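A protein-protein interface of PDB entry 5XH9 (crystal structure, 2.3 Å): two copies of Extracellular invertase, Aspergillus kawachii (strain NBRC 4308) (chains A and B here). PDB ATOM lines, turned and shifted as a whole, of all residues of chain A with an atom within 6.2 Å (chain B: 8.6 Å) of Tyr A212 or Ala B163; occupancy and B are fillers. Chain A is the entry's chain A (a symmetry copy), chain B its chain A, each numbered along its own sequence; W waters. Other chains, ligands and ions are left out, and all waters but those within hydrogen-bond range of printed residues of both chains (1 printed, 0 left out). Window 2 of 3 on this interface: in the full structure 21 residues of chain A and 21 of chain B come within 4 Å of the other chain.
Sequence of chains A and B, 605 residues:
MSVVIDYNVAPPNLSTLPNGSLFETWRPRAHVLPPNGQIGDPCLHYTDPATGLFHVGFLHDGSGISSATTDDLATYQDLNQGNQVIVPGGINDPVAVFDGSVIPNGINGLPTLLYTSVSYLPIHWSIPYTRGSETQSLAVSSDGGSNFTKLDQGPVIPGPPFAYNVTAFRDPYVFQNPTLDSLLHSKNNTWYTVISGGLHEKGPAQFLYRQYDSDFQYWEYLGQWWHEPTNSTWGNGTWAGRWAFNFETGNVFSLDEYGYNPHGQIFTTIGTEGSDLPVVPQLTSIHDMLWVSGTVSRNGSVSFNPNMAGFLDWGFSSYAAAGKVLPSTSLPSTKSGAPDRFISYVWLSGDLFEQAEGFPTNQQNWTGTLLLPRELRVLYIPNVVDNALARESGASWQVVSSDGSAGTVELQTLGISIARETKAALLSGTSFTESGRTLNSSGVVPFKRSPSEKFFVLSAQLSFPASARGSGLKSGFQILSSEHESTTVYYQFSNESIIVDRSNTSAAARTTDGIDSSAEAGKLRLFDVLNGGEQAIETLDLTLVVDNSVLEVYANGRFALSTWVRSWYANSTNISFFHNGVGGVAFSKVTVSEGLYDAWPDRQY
Water W1 lies within hydrogen-bond range of the side-chain hydroxyl of Tyr A218 (2.7 Å) and the backbone carbonyl oxygen of Tyr B164 (2.7 Å).
Of the 11 printed residues of chain B, 4 touch a printed residue of chain A.
Hydrophobic or aromatic side chains of chain B within 4 Å of the printed part of chain A: Phe B162 and Ala B163.
Of the 9 printed residues of chain A, 4 touch a printed residue of chain B.
Hydrophobic or aromatic side chains of chain A within 4 Å of the printed part of chain B: Tyr A212 and Tyr A218.
Tyr A212 touches just these residues of chain B: Phe B162 (3.7 Å) and Ala B163 (3.9 Å).
Printed residues of chain B within 4 Å of Trp A219: Phe B162 (3.2 Å).
Printed residues of chain B within 4 Å of Glu A220: Phe B162.
Pro B161 touches none of the printed residues of chain A.
Of chain A, only Tyr A212 (3.9 Å) and Tyr A218 (3.6 Å) come within 4 Å of Ala B163.
The nearest printed residue of chain A that does not touch Ala B163 is Asp A213 (7.1 Å).
The side-chain carboxylate of Asp A213 is in hydrogen-bond range of the backbone NH of Tyr A218.
N of Tyr A212 lies within hydrogen-bond range of O of Tyr A218 (3.0 Å).
The guanidinium group (NE) of Arg A210 is in salt-bridge range of the side-chain carboxylate (OE1) of Glu A220, at 2.8 Å.
CE2 of Phe B162 touches CD1 of Tyr A212, 3.7 Å away.
Tyr A212 touches Ala B163 (CE2 to CB, 3.9 Å).
CZ of Arg B131 touches CE1 of Tyr A218 (3.4 Å).
Phe B162 touches Tyr A218 (CZ to CB, 3.95 Å).
Ala B163 touches Tyr A218.
OH of Tyr A218 touches O of Tyr B164 (3.9 Å).
Trp A219 touches Phe B162.
CZ of Phe B162 touches CA of Glu A220, 3.6 Å away.
No position is printed for both chains.
Of the 8 pairs that touch across the chains among the printed residues, none has its exchanged pair printed and touching as well.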
ATOM      1  N   LYS A 187      21.080 -19.155   3.384  1.00  0.00           N
ATOM      2  CA  LYS A 187      22.404 -19.657   2.977  1.00  0.00           C
ATOM      3  C   LYS A 187      22.983 -20.503   4.097  1.00  0.00           C
ATOM      4  O   LYS A 187      22.630 -20.302   5.256  1.00  0.00           O
ATOM      5  CB  LYS A 187      23.362 -18.518   2.639  1.00  0.00           C
ATOM      6  CG  LYS A 187      22.809 -17.572   1.583  1.00  0.00           C
ATOM      7  CD  LYS A 187      23.889 -16.794   0.852  1.00  0.00           C
ATOM      8  CE  LYS A 187      23.249 -15.801  -0.115  1.00  0.00           C
ATOM      9  NZ  LYS A 187      24.221 -15.287  -1.116  1.00  0.00           N
ATOM     10  N   ARG A 210      17.595 -12.720  10.509  1.00  0.00           N
ATOM     11  CA  ARG A 210      18.773 -13.326   9.920  1.00  0.00           C
ATOM     12  C   ARG A 210      19.576 -12.286   9.179  1.00  0.00           C
ATOM     13  O   ARG A 210      18.996 -11.335   8.644  1.00  0.00           O
ATOM     14  CB  ARG A 210      18.407 -14.475   8.977  1.00  0.00           C
ATOM     15  CG  ARG A 210      17.644 -14.093   7.728  1.00  0.00           C
ATOM     16  CD  ARG A 210      17.602 -15.238   6.722  1.00  0.00           C
ATOM     17  NE  ARG A 210      16.714 -14.854   5.632  1.00  0.00           N
ATOM     18  CZ  ARG A 210      16.050 -15.683   4.824  1.00  0.00           C
ATOM     19  NH1 ARG A 210      16.156 -17.018   4.920  1.00  0.00           N
ATOM     20  NH2 ARG A 210      15.269 -15.161   3.891  1.00  0.00           N
ATOM     21  N   GLN A 211      20.898 -12.486   9.125  1.00  0.00           N
ATOM     22  CA  GLN A 211      21.764 -11.622   8.330  1.00  0.00           C
ATOM     23  C   GLN A 211      21.290 -11.665   6.864  1.00  0.00           C
ATOM     24  O   GLN A 211      20.965 -12.742   6.340  1.00  0.00           O
ATOM     25  CB  GLN A 211      23.262 -11.983   8.476  1.00  0.00           C
ATOM     26  CG  GLN A 211      23.751 -13.161   7.661  1.00  0.00           C
ATOM     27  CD  GLN A 211      25.245 -13.450   7.786  1.00  0.00           C
ATOM     28  OE1 GLN A 211      26.097 -12.590   7.524  1.00  0.00           O
ATOM     29  NE2 GLN A 211      25.564 -14.687   8.107  1.00  0.00           N
ATOM     30  N   TYR A 212      21.183 -10.481   6.269  1.00  0.00           N
ATOM     31  CA  TYR A 212      20.762 -10.275   4.881  1.00  0.00           C
ATOM     32  C   TYR A 212      21.952 -10.284   3.923  1.00  0.00           C
ATOM     33  O   TYR A 212      21.838 -10.632   2.756  1.00  0.00           O
ATOM     34  CB  TYR A 212      20.072  -8.911   4.787  1.00  0.00           C
ATOM     35  CG  TYR A 212      19.395  -8.620   3.475  1.00  0.00           C
ATOM     36  CD1 TYR A 212      18.186  -9.253   3.149  1.00  0.00           C
ATOM     37  CD2 TYR A 212      19.941  -7.706   2.560  1.00  0.00           C
ATOM     38  CE1 TYR A 212      17.536  -8.989   1.958  1.00  0.00           C
ATOM     39  CE2 TYR A 212      19.300  -7.441   1.353  1.00  0.00           C
ATOM     40  CZ  TYR A 212      18.091  -8.091   1.066  1.00  0.00           C
ATOM     41  OH  TYR A 212      17.413  -7.858  -0.096  1.00  0.00           O
ATOM     42  N   ASP A 213      23.103  -9.914   4.447  1.00  0.00           N
ATOM     43  CA  ASP A 213      24.259  -9.585   3.649  1.00  0.00           C
ATOM     44  C   ASP A 213      25.449 -10.225   4.327  1.00  0.00           C
ATOM     45  O   ASP A 213      25.465 -10.401   5.560  1.00  0.00           O
ATOM     46  CB  ASP A 213      24.428  -8.049   3.610  1.00  0.00           C
ATOM     47  CG  ASP A 213      24.450  -7.400   5.037  1.00  0.00           C
ATOM     48  OD1 ASP A 213      23.518  -7.591   5.842  1.00  0.00           O
ATOM     49  OD2 ASP A 213      25.409  -6.702   5.378  1.00  0.00           O
ATOM     50  N   SER A 214      26.469 -10.543   3.551  1.00  0.00           N
ATOM     51  CA  SER A 214      27.732 -10.930   4.165  1.00  0.00           C
ATOM     52  C   SER A 214      28.275  -9.895   5.200  1.00  0.00           C
ATOM     53  O   SER A 214      29.003 -10.321   6.083  1.00  0.00           O
ATOM     54  CB  SER A 214      28.792 -11.254   3.099  1.00  0.00           C
ATOM     55  OG  SER A 214      28.827 -10.255   2.090  1.00  0.00           O
ATOM     56  N   TYR A 218      22.751  -5.490   7.699  1.00  0.00           N
ATOM     57  CA  TYR A 218      21.301  -5.548   7.650  1.00  0.00           C
ATOM     58  C   TYR A 218      20.803  -6.876   8.195  1.00  0.00           C
ATOM     59  O   TYR A 218      21.384  -7.928   7.921  1.00  0.00           O
ATOM     60  CB  TYR A 218      20.810  -5.301   6.208  1.00  0.00           C
ATOM     61  CG  TYR A 218      21.177  -3.909   5.711  1.00  0.00           C
ATOM     62  CD1 TYR A 218      20.505  -2.785   6.207  1.00  0.00           C
ATOM     63  CD2 TYR A 218      22.195  -3.704   4.752  1.00  0.00           C
ATOM     64  CE1 TYR A 218      20.826  -1.502   5.782  1.00  0.00           C
ATOM     65  CE2 TYR A 218      22.525  -2.410   4.324  1.00  0.00           C
ATOM     66  CZ  TYR A 218      21.832  -1.313   4.860  1.00  0.00           C
ATOM     67  OH  TYR A 218      22.114  -0.014   4.507  1.00  0.00           O
ATOM     68  N   TRP A 219      19.727  -6.811   8.972  1.00  0.00           N
ATOM     69  CA  TRP A 219      19.124  -7.985   9.609  1.00  0.00           C
ATOM     70  C   TRP A 219      17.650  -8.056   9.215  1.00  0.00           C
ATOM     71  O   TRP A 219      16.832  -7.186   9.562  1.00  0.00           O
ATOM     72  CB  TRP A 219      19.329  -7.939  11.142  1.00  0.00           C
ATOM     73  CG  TRP A 219      20.783  -7.983  11.468  1.00  0.00           C
ATOM     74  CD1 TRP A 219      21.650  -6.944  11.427  1.00  0.00           C
ATOM     75  CD2 TRP A 219      21.561  -9.146  11.783  1.00  0.00           C
ATOM     76  NE1 TRP A 219      22.918  -7.373  11.735  1.00  0.00           N
ATOM     77  CE2 TRP A 219      22.893  -8.725  11.942  1.00  0.00           C
ATOM     78  CE3 TRP A 219      21.253 -10.502  11.961  1.00  0.00           C
ATOM     79  CZ2 TRP A 219      23.922  -9.599  12.274  1.00  0.00           C
ATOM     80  CZ3 TRP A 219      22.270 -11.378  12.263  1.00  0.00           C
ATOM     81  CH2 TRP A 219      23.594 -10.926  12.430  1.00  0.00           C
ATOM     82  N   GLU A 220      17.333  -9.091   8.443  1.00  0.00           N
ATOM     83  CA  GLU A 220      16.011  -9.278   7.866  1.00  0.00           C
ATOM     84  C   GLU A 220      15.104  -9.808   8.949  1.00  0.00           C
ATOM     85  O   GLU A 220      15.432 -10.822   9.559  1.00  0.00           O
ATOM     86  CB  GLU A 220      16.101 -10.298   6.722  1.00  0.00           C
ATOM     87  CG  GLU A 220      14.816 -10.522   5.932  1.00  0.00           C
ATOM     88  CD  GLU A 220      14.951 -11.625   4.876  1.00  0.00           C
ATOM     89  OE1 GLU A 220      16.014 -12.261   4.703  1.00  0.00           O
ATOM     90  OE2 GLU A 220      13.952 -11.863   4.207  1.00  0.00           O
ATOM     91  N   ARG B 131      25.713   4.595   7.515  1.00  0.00           N
ATOM     92  CA  ARG B 131      24.439   4.156   8.082  1.00  0.00           C
ATOM     93  C   ARG B 131      24.049   5.025   9.287  1.00  0.00           C
ATOM     94  O   ARG B 131      24.877   5.297  10.137  1.00  0.00           O
ATOM     95  CB  ARG B 131      24.584   2.687   8.512  1.00  0.00           C
ATOM     96  CG  ARG B 131      23.316   2.053   9.086  1.00  0.00           C
ATOM     97  CD  ARG B 131      22.381   1.596   7.986  1.00  0.00           C
ATOM     98  NE  ARG B 131      21.200   0.916   8.516  1.00  0.00           N
ATOM     99  CZ  ARG B 131      21.172  -0.345   8.955  1.00  0.00           C
ATOM    100  NH1 ARG B 131      22.264  -1.086   8.972  1.00  0.00           N
ATOM    101  NH2 ARG B 131      20.040  -0.871   9.390  1.00  0.00           N
ATOM    102  N   GLY B 159      15.697   5.930   9.542  1.00  0.00           N
ATOM    103  CA  GLY B 159      16.501   5.631   8.372  1.00  0.00           C
ATOM    104  C   GLY B 159      15.693   5.299   7.143  1.00  0.00           C
ATOM    105  O   GLY B 159      14.449   5.253   7.184  1.00  0.00           O
ATOM    106  N   PRO B 160      16.382   5.093   6.023  1.00  0.00           N
ATOM    107  CA  PRO B 160      15.688   4.722   4.800  1.00  0.00           C
ATOM    108  C   PRO B 160      15.146   3.310   4.905  1.00  0.00           C
ATOM    109  O   PRO B 160      15.509   2.598   5.833  1.00  0.00           O
ATOM    110  CB  PRO B 160      16.790   4.766   3.738  1.00  0.00           C
ATOM    111  CG  PRO B 160      18.058   4.568   4.496  1.00  0.00           C
ATOM    112  CD  PRO B 160      17.841   5.171   5.844  1.00  0.00           C
ATOM    113  N   PRO B 161      14.303   2.895   3.953  1.00  0.00           N
ATOM    114  CA  PRO B 161      13.750   1.532   3.951  1.00  0.00           C
ATOM    115  C   PRO B 161      14.842   0.466   3.925  1.00  0.00           C
ATOM    116  O   PRO B 161      15.968   0.736   3.484  1.00  0.00           O
ATOM    117  CB  PRO B 161      12.947   1.478   2.635  1.00  0.00           C
ATOM    118  CG  PRO B 161      12.651   2.917   2.315  1.00  0.00           C
ATOM    119  CD  PRO B 161      13.876   3.650   2.757  1.00  0.00           C
ATOM    120  N   PHE B 162      14.468  -0.733   4.356  1.00  0.00           N
ATOM    121  CA  PHE B 162      15.388  -1.822   4.646  1.00  0.00           C
ATOM    122  C   PHE B 162      16.406  -2.069   3.517  1.00  0.00           C
ATOM    123  O   PHE B 162      16.020  -2.255   2.379  1.00  0.00           O
ATOM    124  CB  PHE B 162      14.578  -3.097   4.948  1.00  0.00           C
ATOM    125  CG  PHE B 162      15.433  -4.286   5.281  1.00  0.00           C
ATOM    126  CD1 PHE B 162      16.059  -4.386   6.533  1.00  0.00           C
ATOM    127  CD2 PHE B 162      15.631  -5.309   4.346  1.00  0.00           C
ATOM    128  CE1 PHE B 162      16.856  -5.480   6.843  1.00  0.00           C
ATOM    129  CE2 PHE B 162      16.433  -6.401   4.655  1.00  0.00           C
ATOM    130  CZ  PHE B 162      17.049  -6.483   5.901  1.00  0.00           C
ATOM    131  N   ALA B 163      17.701  -2.017   3.843  1.00  0.00           N
ATOM    132  CA  ALA B 163      18.812  -2.265   2.890  1.00  0.00           C
ATOM    133  C   ALA B 163      18.988  -1.278   1.730  1.00  0.00           C
ATOM    134  O   ALA B 163      19.794  -1.543   0.855  1.00  0.00           O
ATOM    135  CB  ALA B 163      18.760  -3.704   2.344  1.00  0.00           C
ATOM    136  N   TYR B 164      18.274  -0.151   1.716  1.00  0.00           N
ATOM    137  CA  TYR B 164      18.440   0.835   0.626  1.00  0.00           C
ATOM    138  C   TYR B 164      19.780   1.525   0.792  1.00  0.00           C
ATOM    139  O   TYR B 164      20.088   2.000   1.882  1.00  0.00           O
ATOM    140  CB  TYR B 164      17.309   1.885   0.636  1.00  0.00           C
ATOM    141  CG  TYR B 164      16.006   1.470  -0.037  1.00  0.00           C
ATOM    142  CD1 TYR B 164      15.642   0.123  -0.177  1.00  0.00           C
ATOM    143  CD2 TYR B 164      15.125   2.439  -0.525  1.00  0.00           C
ATOM    144  CE1 TYR B 164      14.445  -0.234  -0.791  1.00  0.00           C
ATOM    145  CE2 TYR B 164      13.926   2.089  -1.131  1.00  0.00           C
ATOM    146  CZ  TYR B 164      13.591   0.756  -1.275  1.00  0.00           C
ATOM    147  OH  TYR B 164      12.406   0.403  -1.874  1.00  0.00           O
ATOM    148  N   ASN B 165      20.579   1.536  -0.273  1.00  0.00           N
ATOM    149  CA  ASN B 165      21.896   2.187  -0.291  1.00  0.00           C
ATOM    150  C   ASN B 165      21.708   3.633  -0.819  1.00  0.00           C
ATOM    151  O   ASN B 165      21.941   3.937  -2.010  1.00  0.00           O
ATOM    152  CB  ASN B 165      22.896   1.393  -1.152  1.00  0.00           C
ATOM    153  CG  ASN B 165      24.302   1.998  -1.131  1.00  0.00           C
ATOM    154  OD1 ASN B 165      24.580   2.900  -0.360  1.00  0.00           O
ATOM    155  ND2 ASN B 165      25.185   1.509  -1.996  1.00  0.00           N
ATOM    156  N   VAL B 166      21.251   4.505   0.078  1.00  0.00           N
ATOM    157  CA  VAL B 166      20.950   5.875  -0.271  1.00  0.00           C
ATOM    158  C   VAL B 166      22.200   6.716  -0.514  1.00  0.00           C
ATOM    159  O   VAL B 166      23.227   6.481   0.100  1.00  0.00           O
ATOM    160  CB  VAL B 166      20.090   6.577   0.793  1.00  0.00           C
ATOM    161  CG1 VAL B 166      18.705   5.935   0.871  1.00  0.00           C
ATOM    162  CG2 VAL B 166      20.801   6.625   2.154  1.00  0.00           C
ATOM    163  N   LEU B 199      19.501   6.933  -4.680  1.00  0.00           N
ATOM    164  CA  LEU B 199      20.095   5.610  -4.480  1.00  0.00           C
ATOM    165  C   LEU B 199      21.341   5.465  -5.350  1.00  0.00           C
ATOM    166  O   LEU B 199      21.311   5.786  -6.538  1.00  0.00           O
ATOM    167  CB  LEU B 199      19.061   4.513  -4.784  1.00  0.00           C
ATOM    168  CG  LEU B 199      17.826   4.467  -3.880  1.00  0.00           C
ATOM    169  CD1 LEU B 199      16.834   3.436  -4.401  1.00  0.00           C
ATOM    170  CD2 LEU B 199      18.202   4.108  -2.446  1.00  0.00           C
ATOM    171  N   LYS B 202      21.430   3.773  -8.996  1.00  0.00           N
ATOM    172  CA  LYS B 202      20.074   3.861  -9.560  1.00  0.00           C
ATOM    173  C   LYS B 202      19.770   5.297  -9.939  1.00  0.00           C
ATOM    174  O   LYS B 202      19.523   5.566 -11.107  1.00  0.00           O
ATOM    175  CB  LYS B 202      19.002   3.290  -8.619  1.00  0.00           C
ATOM    176  CG  LYS B 202      19.168   1.793  -8.371  1.00  0.00           C
ATOM    177  CD  LYS B 202      17.887   1.096  -7.916  1.00  0.00           C
ATOM    178  CE  LYS B 202      18.118  -0.414  -7.768  1.00  0.00           C
ATOM    179  NZ  LYS B 202      17.050  -1.119  -6.995  1.00  0.00           N
HETATM  180  O   HOH W   1      20.009   1.606   4.586  1.00  0.00           O
